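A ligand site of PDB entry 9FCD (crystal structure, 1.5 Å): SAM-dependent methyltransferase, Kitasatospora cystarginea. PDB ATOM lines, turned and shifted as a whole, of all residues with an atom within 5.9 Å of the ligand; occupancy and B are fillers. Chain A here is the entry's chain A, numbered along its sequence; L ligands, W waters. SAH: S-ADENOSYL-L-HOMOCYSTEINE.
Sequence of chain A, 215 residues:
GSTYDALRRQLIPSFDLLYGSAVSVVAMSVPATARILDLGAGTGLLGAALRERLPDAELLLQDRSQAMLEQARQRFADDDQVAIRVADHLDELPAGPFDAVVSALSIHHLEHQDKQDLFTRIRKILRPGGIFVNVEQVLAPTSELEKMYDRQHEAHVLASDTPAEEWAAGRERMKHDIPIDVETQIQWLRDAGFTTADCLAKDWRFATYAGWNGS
The backbone NH (N) of Arg 64 sits at hydrogen-bond distance from a nitrogen (N3) of the ligand (3.4 Å).
A ring nitrogen (ND1) of His 89 lies close to a nitrogen (N1) of the ligand, at 3.5 Å.
An oxygen (O4') of the ligand sits at hydrogen-bond distance from the side-chain hydroxyl of Ser 106, at 2.8 Å.
The side-chain carboxylate (OD1) of Asp 63 sits at hydrogen-bond distance from an oxygen (O3') of the ligand, at 2.7 Å.
N1 of the ligand sits at hydrogen-bond distance from N of His 89, at 2.9 Å.
O of Ala 104 is in hydrogen-bond range of N of the ligand, at 2.9 Å.
O of Gly 40 sits at hydrogen-bond distance from N of the ligand (2.9 Å).
An oxygen (O) of the ligand sits at hydrogen-bond distance from the side-chain hydroxyl of Tyr 19, 2.6 Å away.
The side-chain carboxylate (OD1) of Asp 88 sits at hydrogen-bond distance from a nitrogen (N6) of the ligand (3.0 Å).
Water W1 lies within hydrogen-bond range of OXT of the ligand, OG1 of Thr 43 and OH of Tyr 4.
Water W4 lies within hydrogen-bond range of OXT of the ligand (2.7 Å), NE of Arg 8 (2.8 Å) and OH of Tyr 19 (2.9 Å).
Water W2 lies within hydrogen-bond range of the guanidinium group (NE) of Arg 64 and an oxygen (O2') of the ligand.
Water W6 lies within hydrogen-bond range of the backbone carbonyl oxygen (O) of Ala 41 (2.7 Å), the side-chain carboxylate (OD2) of Asp 38 (2.8 Å), the backbone NH (N) of Leu 46 (3.0 Å), a nitrogen (N) of the ligand (3.1 Å) and the backbone NH (N) of Leu 45 (3.5 Å).
Water W5 lies within hydrogen-bond range of OD2 of Asp 88 (2.5 Å), NH1 of Arg 64 (2.6 Å) and N6 of the ligand (3.4 Å).
SD of the ligand lies close to O of Leu 105 (3.7 Å).
Ala 41 touches the ligand.
Gly 42 touches the ligand (CA to O3', 3.1 Å).
CD1 of Leu 45 touches OXT of the ligand, 3.8 Å away.
Ser 65 touches the ligand (CB to O2', 3.8 Å).
CE of Met 68 touches O3' of the ligand, at 3.5 Å.
Ala 87 touches the ligand.
ND1 of His 109 touches C8 of the ligand, 3.8 Å away.
Leu 110 touches the ligand (CD2 to N6, 3.8 Å).
Hydrophobic or aromatic side chains that line the ligand: Tyr 19, Leu 45, Met 68, His 89, Ala 104, His 109 and Leu 110.
Of the 27 residues printed, 17 come within 4 Å of the ligand.
The nearest printed residue that does not touch the ligand is Tyr 4 (4.4 Å).
The backbone NH (N) of Ala 41 sits at hydrogen-bond distance from the side-chain carboxylate (OD1) of Asp 63 (3.4 Å).
The side-chain hydroxyl of Ser 65 sits at hydrogen-bond distance from the backbone NH of Met 68 (3.0 Å).
The backbone NH (N) of Gly 42 sits at hydrogen-bond distance from the side-chain carboxylate (OD1) of Asp 63, at 2.8 Å.
O of Asp 63 sits at hydrogen-bond distance from N of Ala 87 (3.0 Å).
O of Gln 62 lies within hydrogen-bond range of N of Ala 41, at 2.9 Å.
The backbone NH (N) of Arg 64 sits at hydrogen-bond distance from the backbone carbonyl oxygen (O) of Ala 87.
The backbone NH (N) of Gly 40 lies within hydrogen-bond range of the backbone carbonyl oxygen (O) of Gln 62 (2.8 Å).
N of Ser 65 is in hydrogen-bond range of OD2 of Asp 63 (2.9 Å).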
ATOM      1  N   TYR A   4     -13.970  -2.788   1.247  1.00  0.00           N
ATOM      2  CA  TYR A   4     -14.337  -2.921  -0.187  1.00  0.00           C
ATOM      3  C   TYR A   4     -15.592  -3.788  -0.314  1.00  0.00           C
ATOM      4  O   TYR A   4     -16.547  -3.356  -0.975  1.00  0.00           O
ATOM      5  CB  TYR A   4     -13.195  -3.530  -1.013  1.00  0.00           C
ATOM      6  CG  TYR A   4     -13.583  -3.726  -2.455  1.00  0.00           C
ATOM      7  CD1 TYR A   4     -13.437  -2.706  -3.389  1.00  0.00           C
ATOM      8  CD2 TYR A   4     -14.161  -4.915  -2.881  1.00  0.00           C
ATOM      9  CE1 TYR A   4     -13.815  -2.877  -4.704  1.00  0.00           C
ATOM     10  CE2 TYR A   4     -14.541  -5.099  -4.202  1.00  0.00           C
ATOM     11  CZ  TYR A   4     -14.371  -4.076  -5.113  1.00  0.00           C
ATOM     12  OH  TYR A   4     -14.745  -4.245  -6.415  1.00  0.00           O
ATOM     13  N   ARG A   8     -19.448  -2.863  -1.614  1.00  0.00           N
ATOM     14  CA  ARG A   8     -20.161  -3.541  -2.722  1.00  0.00           C
ATOM     15  C   ARG A   8     -21.587  -3.886  -2.276  1.00  0.00           C
ATOM     16  O   ARG A   8     -22.523  -3.687  -3.087  1.00  0.00           O
ATOM     17  CB  ARG A   8     -19.380  -4.778  -3.199  1.00  0.00           C
ATOM     18  CG  ARG A   8     -18.025  -4.462  -3.799  1.00  0.00           C
ATOM     19  CD  ARG A   8     -18.057  -3.365  -4.851  1.00  0.00           C
ATOM     20  NE  ARG A   8     -18.756  -3.787  -6.048  1.00  0.00           N
ATOM     21  CZ  ARG A   8     -19.038  -3.007  -7.087  1.00  0.00           C
ATOM     22  NH1 ARG A   8     -18.701  -1.733  -7.066  1.00  0.00           N
ATOM     23  NH2 ARG A   8     -19.671  -3.512  -8.136  1.00  0.00           N
ATOM     24  N   TYR A  19     -25.796 -12.908  -5.684  1.00  0.00           N
ATOM     25  CA  TYR A  19     -24.523 -13.672  -5.698  1.00  0.00           C
ATOM     26  C   TYR A  19     -24.791 -15.082  -5.189  1.00  0.00           C
ATOM     27  O   TYR A  19     -24.260 -16.050  -5.761  1.00  0.00           O
ATOM     28  CB  TYR A  19     -23.432 -12.950  -4.903  1.00  0.00           C
ATOM     29  CG  TYR A  19     -22.733 -11.839  -5.649  1.00  0.00           C
ATOM     30  CD1 TYR A  19     -21.439 -11.998  -6.096  1.00  0.00           C
ATOM     31  CD2 TYR A  19     -23.366 -10.635  -5.907  1.00  0.00           C
ATOM     32  CE1 TYR A  19     -20.773 -10.986  -6.776  1.00  0.00           C
ATOM     33  CE2 TYR A  19     -22.720  -9.624  -6.596  1.00  0.00           C
ATOM     34  CZ  TYR A  19     -21.425  -9.794  -7.035  1.00  0.00           C
ATOM     35  OH  TYR A  19     -20.785  -8.777  -7.679  1.00  0.00           O
ATOM     36  N   ASP A  38     -14.183 -17.311 -14.081  1.00  0.00           N
ATOM     37  CA  ASP A  38     -14.856 -16.072 -13.625  1.00  0.00           C
ATOM     38  C   ASP A  38     -14.384 -14.950 -14.556  1.00  0.00           C
ATOM     39  O   ASP A  38     -13.217 -14.556 -14.423  1.00  0.00           O
ATOM     40  CB  ASP A  38     -14.562 -15.821 -12.136  1.00  0.00           C
ATOM     41  CG  ASP A  38     -15.307 -14.651 -11.519  1.00  0.00           C
ATOM     42  OD1 ASP A  38     -16.145 -14.063 -12.223  1.00  0.00           O
ATOM     43  OD2 ASP A  38     -15.032 -14.338 -10.335  1.00  0.00           O
ATOM     44  N   LEU A  39     -15.250 -14.505 -15.470  1.00  0.00           N
ATOM     45  CA  LEU A  39     -14.955 -13.452 -16.477  1.00  0.00           C
ATOM     46  C   LEU A  39     -15.163 -12.071 -15.853  1.00  0.00           C
ATOM     47  O   LEU A  39     -16.276 -11.816 -15.342  1.00  0.00           O
ATOM     48  CB  LEU A  39     -15.897 -13.592 -17.669  1.00  0.00           C
ATOM     49  CG  LEU A  39     -15.608 -14.704 -18.667  1.00  0.00           C
ATOM     50  CD1 LEU A  39     -16.686 -14.724 -19.729  1.00  0.00           C
ATOM     51  CD2 LEU A  39     -14.242 -14.513 -19.283  1.00  0.00           C
ATOM     52  N   GLY A  40     -14.188 -11.190 -15.978  1.00  0.00           N
ATOM     53  CA  GLY A  40     -14.267  -9.855 -15.338  1.00  0.00           C
ATOM     54  C   GLY A  40     -14.344 -10.006 -13.838  1.00  0.00           C
ATOM     55  O   GLY A  40     -15.138  -9.307 -13.197  1.00  0.00           O
ATOM     56  N   ALA A  41     -13.491 -10.868 -13.278  1.00  0.00           N
ATOM     57  CA  ALA A  41     -13.522 -11.310 -11.868  1.00  0.00           C
ATOM     58  C   ALA A  41     -13.259 -10.156 -10.904  1.00  0.00           C
ATOM     59  O   ALA A  41     -13.562 -10.312  -9.719  1.00  0.00           O
ATOM     60  CB  ALA A  41     -12.503 -12.392 -11.677  1.00  0.00           C
ATOM     61  N   GLY A  42     -12.640  -9.066 -11.361  1.00  0.00           N
ATOM     62  CA  GLY A  42     -12.284  -7.930 -10.478  1.00  0.00           C
ATOM     63  C   GLY A  42     -11.465  -8.397  -9.283  1.00  0.00           C
ATOM     64  O   GLY A  42     -10.415  -9.038  -9.498  1.00  0.00           O
ATOM     65  N   THR A  43     -11.886  -8.065  -8.072  1.00  0.00           N
ATOM     66  CA  THR A  43     -11.197  -8.455  -6.816  1.00  0.00           C
ATOM     67  C   THR A  43     -11.494  -9.914  -6.462  1.00  0.00           C
ATOM     68  O   THR A  43     -11.000 -10.378  -5.418  1.00  0.00           O
ATOM     69  CB  THR A  43     -11.568  -7.528  -5.654  1.00  0.00           C
ATOM     70  OG1 THR A  43     -12.905  -7.833  -5.259  1.00  0.00           O
ATOM     71  CG2 THR A  43     -11.442  -6.066  -5.978  1.00  0.00           C
ATOM     72  N   GLY A  44     -12.323 -10.602  -7.258  1.00  0.00           N
ATOM     73  CA  GLY A  44     -12.594 -12.045  -7.104  1.00  0.00           C
ATOM     74  C   GLY A  44     -13.774 -12.353  -6.198  1.00  0.00           C
ATOM     75  O   GLY A  44     -13.841 -13.490  -5.726  1.00  0.00           O
ATOM     76  N   LEU A  45     -14.720 -11.433  -6.026  1.00  0.00           N
ATOM     77  CA  LEU A  45     -15.875 -11.627  -5.104  1.00  0.00           C
ATOM     78  C   LEU A  45     -16.726 -12.821  -5.524  1.00  0.00           C
ATOM     79  O   LEU A  45     -17.134 -13.581  -4.636  1.00  0.00           O
ATOM     80  CB  LEU A  45     -16.729 -10.358  -5.047  1.00  0.00           C
ATOM     81  CG  LEU A  45     -16.470  -9.425  -3.875  1.00  0.00           C
ATOM     82  CD1 LEU A  45     -17.371  -8.205  -3.968  1.00  0.00           C
ATOM     83  CD2 LEU A  45     -16.691 -10.138  -2.549  1.00  0.00           C
ATOM     84  N   LEU A  46     -17.063 -12.966  -6.801  1.00  0.00           N
ATOM     85  CA  LEU A  46     -17.928 -14.109  -7.232  1.00  0.00           C
ATOM     86  C   LEU A  46     -17.132 -15.416  -7.077  1.00  0.00           C
ATOM     87  O   LEU A  46     -17.696 -16.386  -6.555  1.00  0.00           O
ATOM     88  CB  LEU A  46     -18.431 -13.900  -8.653  1.00  0.00           C
ATOM     89  CG  LEU A  46     -19.375 -14.984  -9.166  1.00  0.00           C
ATOM     90  CD1 LEU A  46     -20.539 -15.222  -8.206  1.00  0.00           C
ATOM     91  CD2 LEU A  46     -19.895 -14.642 -10.549  1.00  0.00           C
ATOM     92  N   GLN A  62     -10.296 -14.140 -14.455  1.00  0.00           N
ATOM     93  CA  GLN A  62      -9.809 -13.374 -15.616  1.00  0.00           C
ATOM     94  C   GLN A  62     -10.366 -11.962 -15.553  1.00  0.00           C
ATOM     95  O   GLN A  62     -11.551 -11.795 -15.239  1.00  0.00           O
ATOM     96  CB  GLN A  62     -10.229 -14.073 -16.901  1.00  0.00           C
ATOM     97  CG  GLN A  62      -9.724 -13.375 -18.145  1.00  0.00           C
ATOM     98  CD  GLN A  62     -10.084 -14.206 -19.348  1.00  0.00           C
ATOM     99  OE1 GLN A  62      -9.550 -15.299 -19.551  1.00  0.00           O
ATOM    100  NE2 GLN A  62     -10.987 -13.682 -20.160  1.00  0.00           N
ATOM    101  N   ASP A  63      -9.535 -10.976 -15.875  1.00  0.00           N
ATOM    102  CA  ASP A  63      -9.959  -9.553 -15.922  1.00  0.00           C
ATOM    103  C   ASP A  63      -8.969  -8.795 -16.801  1.00  0.00           C
ATOM    104  O   ASP A  63      -7.829  -9.256 -16.939  1.00  0.00           O
ATOM    105  CB  ASP A  63     -10.027  -8.965 -14.507  1.00  0.00           C
ATOM    106  CG  ASP A  63     -10.920  -7.739 -14.390  1.00  0.00           C
ATOM    107  OD1 ASP A  63     -12.046  -7.894 -13.864  1.00  0.00           O
ATOM    108  OD2 ASP A  63     -10.478  -6.639 -14.793  1.00  0.00           O
ATOM    109  N   ARG A  64      -9.392  -7.651 -17.343  1.00  0.00           N
ATOM    110  CA  ARG A  64      -8.462  -6.804 -18.137  1.00  0.00           C
ATOM    111  C   ARG A  64      -7.526  -6.037 -17.189  1.00  0.00           C
ATOM    112  O   ARG A  64      -6.453  -5.619 -17.647  1.00  0.00           O
ATOM    113  CB  ARG A  64      -9.221  -5.848 -19.059  1.00  0.00           C
ATOM    114  CG  ARG A  64      -9.986  -4.745 -18.325  1.00  0.00           C
ATOM    115  CD  ARG A  64     -10.747  -3.803 -19.252  1.00  0.00           C
ATOM    116  NE  ARG A  64     -11.507  -2.845 -18.462  1.00  0.00           N
ATOM    117  CZ  ARG A  64     -12.291  -1.891 -18.950  1.00  0.00           C
ATOM    118  NH1 ARG A  64     -12.425  -1.737 -20.255  1.00  0.00           N
ATOM    119  NH2 ARG A  64     -12.938  -1.076 -18.127  1.00  0.00           N
ATOM    120  N   SER A  65      -7.899  -5.858 -15.919  1.00  0.00           N
ATOM    121  CA  SER A  65      -7.195  -4.935 -14.982  1.00  0.00           C
ATOM    122  C   SER A  65      -6.270  -5.705 -14.041  1.00  0.00           C
ATOM    123  O   SER A  65      -6.766  -6.440 -13.170  1.00  0.00           O
ATOM    124  CB  SER A  65      -8.169  -4.100 -14.201  1.00  0.00           C
ATOM    125  OG  SER A  65      -7.506  -3.417 -13.148  1.00  0.00           O
ATOM    126  N   MET A  68      -7.124  -4.636 -10.402  1.00  0.00           N
ATOM    127  CA  MET A  68      -8.243  -5.408  -9.811  1.00  0.00           C
ATOM    128  C   MET A  68      -7.753  -6.813  -9.444  1.00  0.00           C
ATOM    129  O   MET A  68      -8.001  -7.269  -8.315  1.00  0.00           O
ATOM    130  CB  MET A  68      -9.434  -5.475 -10.777  1.00  0.00           C
ATOM    131  CG  MET A  68     -10.068  -4.111 -11.049  1.00  0.00           C
ATOM    132  SD  MET A  68     -10.820  -3.352  -9.572  1.00  0.00           S
ATOM    133  CE  MET A  68     -12.223  -4.447  -9.350  1.00  0.00           C
ATOM    134  N   ALA A  87      -6.788 -10.746 -19.273  1.00  0.00           N
ATOM    135  CA  ALA A  87      -7.396 -10.770 -20.613  1.00  0.00           C
ATOM    136  C   ALA A  87      -8.665  -9.930 -20.618  1.00  0.00           C
ATOM    137  O   ALA A  87      -9.486 -10.041 -19.685  1.00  0.00           O
ATOM    138  CB  ALA A  87      -7.691 -12.191 -21.032  1.00  0.00           C
ATOM    139  N   ASP A  88      -8.820  -9.135 -21.678  1.00  0.00           N
ATOM    140  CA  ASP A  88     -10.094  -8.464 -22.005  1.00  0.00           C
ATOM    141  C   ASP A  88     -11.108  -9.540 -22.420  1.00  0.00           C
ATOM    142  O   ASP A  88     -10.700 -10.568 -22.973  1.00  0.00           O
ATOM    143  CB  ASP A  88      -9.872  -7.456 -23.127  1.00  0.00           C
ATOM    144  CG  ASP A  88     -10.952  -6.398 -23.181  1.00  0.00           C
ATOM    145  OD1 ASP A  88     -12.055  -6.719 -23.672  1.00  0.00           O
ATOM    146  OD2 ASP A  88     -10.678  -5.275 -22.703  1.00  0.00           O
ATOM    147  N   HIS A  89     -12.402  -9.285 -22.214  1.00  0.00           N
ATOM    148  CA  HIS A  89     -13.474 -10.164 -22.757  1.00  0.00           C
ATOM    149  C   HIS A  89     -13.281 -10.335 -24.261  1.00  0.00           C
ATOM    150  O   HIS A  89     -13.720 -11.363 -24.789  1.00  0.00           O
ATOM    151  CB  HIS A  89     -14.874  -9.608 -22.504  1.00  0.00           C
ATOM    152  CG  HIS A  89     -15.186  -9.308 -21.075  1.00  0.00           C
ATOM    153  ND1 HIS A  89     -14.650 -10.024 -20.030  1.00  0.00           N
ATOM    154  CD2 HIS A  89     -15.988  -8.368 -20.538  1.00  0.00           C
ATOM    155  CE1 HIS A  89     -15.119  -9.538 -18.902  1.00  0.00           C
ATOM    156  NE2 HIS A  89     -15.942  -8.523 -19.180  1.00  0.00           N
ATOM    157  N   LEU A  90     -12.726  -9.327 -24.932  1.00  0.00           N
ATOM    158  CA  LEU A  90     -12.570  -9.317 -26.413  1.00  0.00           C
ATOM    159  C   LEU A  90     -11.260  -9.976 -26.842  1.00  0.00           C
ATOM    160  O   LEU A  90     -11.097 -10.145 -28.050  1.00  0.00           O
ATOM    161  CB  LEU A  90     -12.650  -7.868 -26.909  1.00  0.00           C
ATOM    162  CG  LEU A  90     -13.951  -7.137 -26.588  1.00  0.00           C
ATOM    163  CD1 LEU A  90     -13.979  -5.776 -27.264  1.00  0.00           C
ATOM    164  CD2 LEU A  90     -15.154  -7.967 -27.000  1.00  0.00           C
ATOM    165  N   SER A 103     -19.874 -14.698 -14.345  1.00  0.00           N
ATOM    166  CA  SER A 103     -19.487 -13.275 -14.445  1.00  0.00           C
ATOM    167  C   SER A 103     -20.392 -12.471 -13.530  1.00  0.00           C
ATOM    168  O   SER A 103     -21.558 -12.854 -13.362  1.00  0.00           O
ATOM    169  CB  SER A 103     -19.570 -12.800 -15.880  1.00  0.00           C
ATOM    170  OG  SER A 103     -18.910 -11.551 -16.037  1.00  0.00           O
ATOM    171  N   ALA A 104     -19.859 -11.394 -12.945  1.00  0.00           N
ATOM    172  CA  ALA A 104     -20.693 -10.462 -12.162  1.00  0.00           C
ATOM    173  C   ALA A 104     -20.331  -9.018 -12.539  1.00  0.00           C
ATOM    174  O   ALA A 104     -19.159  -8.644 -12.434  1.00  0.00           O
ATOM    175  CB  ALA A 104     -20.539 -10.720 -10.679  1.00  0.00           C
ATOM    176  N   LEU A 105     -21.339  -8.269 -12.976  1.00  0.00           N
ATOM    177  CA  LEU A 105     -21.302  -6.791 -13.138  1.00  0.00           C
ATOM    178  C   LEU A 105     -20.130  -6.392 -14.040  1.00  0.00           C
ATOM    179  O   LEU A 105     -19.463  -5.390 -13.753  1.00  0.00           O
ATOM    180  CB  LEU A 105     -21.198  -6.144 -11.755  1.00  0.00           C
ATOM    181  CG  LEU A 105     -22.315  -6.508 -10.784  1.00  0.00           C
ATOM    182  CD1 LEU A 105     -22.080  -5.892  -9.423  1.00  0.00           C
ATOM    183  CD2 LEU A 105     -23.672  -6.090 -11.335  1.00  0.00           C
ATOM    184  N   SER A 106     -19.944  -7.109 -15.152  1.00  0.00           N
ATOM    185  CA  SER A 106     -18.806  -6.866 -16.075  1.00  0.00           C
ATOM    186  C   SER A 106     -19.279  -6.779 -17.525  1.00  0.00           C
ATOM    187  O   SER A 106     -18.780  -5.916 -18.259  1.00  0.00           O
ATOM    188  CB  SER A 106     -17.783  -7.945 -15.893  1.00  0.00           C
ATOM    189  OG  SER A 106     -16.596  -7.653 -16.608  1.00  0.00           O
ATOM    190  N   HIS A 109     -20.421  -3.753 -19.750  1.00  0.00           N
ATOM    191  CA  HIS A 109     -19.431  -2.758 -20.262  1.00  0.00           C
ATOM    192  C   HIS A 109     -19.197  -2.924 -21.770  1.00  0.00           C
ATOM    193  O   HIS A 109     -18.611  -2.006 -22.379  1.00  0.00           O
ATOM    194  CB  HIS A 109     -18.133  -2.828 -19.468  1.00  0.00           C
ATOM    195  CG  HIS A 109     -18.296  -2.315 -18.085  1.00  0.00           C
ATOM    196  ND1 HIS A 109     -18.244  -3.134 -16.986  1.00  0.00           N
ATOM    197  CD2 HIS A 109     -18.599  -1.076 -17.631  1.00  0.00           C
ATOM    198  CE1 HIS A 109     -18.457  -2.434 -15.902  1.00  0.00           C
ATOM    199  NE2 HIS A 109     -18.685  -1.166 -16.261  1.00  0.00           N
ATOM    200  N   LEU A 110     -19.635  -4.046 -22.353  1.00  0.00           N
ATOM    201  CA  LEU A 110     -19.446  -4.356 -23.792  1.00  0.00           C
ATOM    202  C   LEU A 110     -20.589  -3.765 -24.615  1.00  0.00           C
ATOM    203  O   LEU A 110     -21.734  -3.726 -24.111  1.00  0.00           O
ATOM    204  CB  LEU A 110     -19.408  -5.873 -23.999  1.00  0.00           C
ATOM    205  CG  LEU A 110     -18.260  -6.611 -23.327  1.00  0.00           C
ATOM    206  CD1 LEU A 110     -18.362  -8.101 -23.596  1.00  0.00           C
ATOM    207  CD2 LEU A 110     -16.913  -6.078 -23.776  1.00  0.00           C
HETATM  208  N   SAH L   1     -16.817  -9.418 -10.886  1.00  0.00           N
HETATM  209  CA  SAH L   1     -16.301  -8.521  -9.822  1.00  0.00           C
HETATM  210  CB  SAH L   1     -15.947  -7.147 -10.386  1.00  0.00           C
HETATM  211  CG  SAH L   1     -17.123  -6.337 -10.920  1.00  0.00           C
HETATM  212  SD  SAH L   1     -16.613  -4.687 -11.459  1.00  0.00           S
HETATM  213  C   SAH L   1     -17.336  -8.388  -8.703  1.00  0.00           C
HETATM  214  O   SAH L   1     -18.410  -8.999  -8.802  1.00  0.00           O
HETATM  215  OXT SAH L   1     -17.103  -7.681  -7.723  1.00  0.00           O
HETATM  216  C5' SAH L   1     -16.366  -4.917 -13.235  1.00  0.00           C
HETATM  217  C4' SAH L   1     -15.077  -5.629 -13.599  1.00  0.00           C
HETATM  218  O4' SAH L   1     -15.095  -5.851 -15.018  1.00  0.00           O
HETATM  219  C3' SAH L   1     -13.783  -4.853 -13.293  1.00  0.00           C
HETATM  220  O3' SAH L   1     -12.858  -5.672 -12.596  1.00  0.00           O
HETATM  221  C2' SAH L   1     -13.282  -4.441 -14.682  1.00  0.00           C
HETATM  222  O2' SAH L   1     -11.877  -4.334 -14.774  1.00  0.00           O
HETATM  223  C1' SAH L   1     -13.814  -5.590 -15.532  1.00  0.00           C
HETATM  224  N9  SAH L   1     -13.952  -5.313 -16.955  1.00  0.00           N
HETATM  225  C8  SAH L   1     -14.700  -4.317 -17.539  1.00  0.00           C
HETATM  226  N7  SAH L   1     -14.675  -4.357 -18.853  1.00  0.00           N
HETATM  227  C5  SAH L   1     -13.897  -5.459 -19.149  1.00  0.00           C
HETATM  228  C6  SAH L   1     -13.503  -6.052 -20.369  1.00  0.00           C
HETATM  229  N6  SAH L   1     -13.873  -5.593 -21.556  1.00  0.00           N
HETATM  230  N1  SAH L   1     -12.733  -7.165 -20.306  1.00  0.00           N
HETATM  231  C2  SAH L   1     -12.370  -7.630 -19.102  1.00  0.00           C
HETATM  232  N3  SAH L   1     -12.674  -7.169 -17.888  1.00  0.00           N
HETATM  233  C4  SAH L   1     -13.452  -6.073 -17.982  1.00  0.00           C
HETATM  234  O   HOH W   1     -14.591  -6.974  -7.295  1.00  0.00           O
HETATM  235  O   HOH W   2     -10.846  -2.170 -16.021  1.00  0.00           O
HETATM  236  O   HOH W   3     -17.001 -11.646 -12.606  1.00  0.00           O
HETATM  237  O   HOH W   4     -19.298  -6.436  -6.902  1.00  0.00           O
HETATM  238  O   HOH W   5     -11.831  -3.019 -22.447  1.00  0.00           O
HETATM  239  O   HOH W   6     -15.784 -11.869  -9.322  1.00  0.00           O
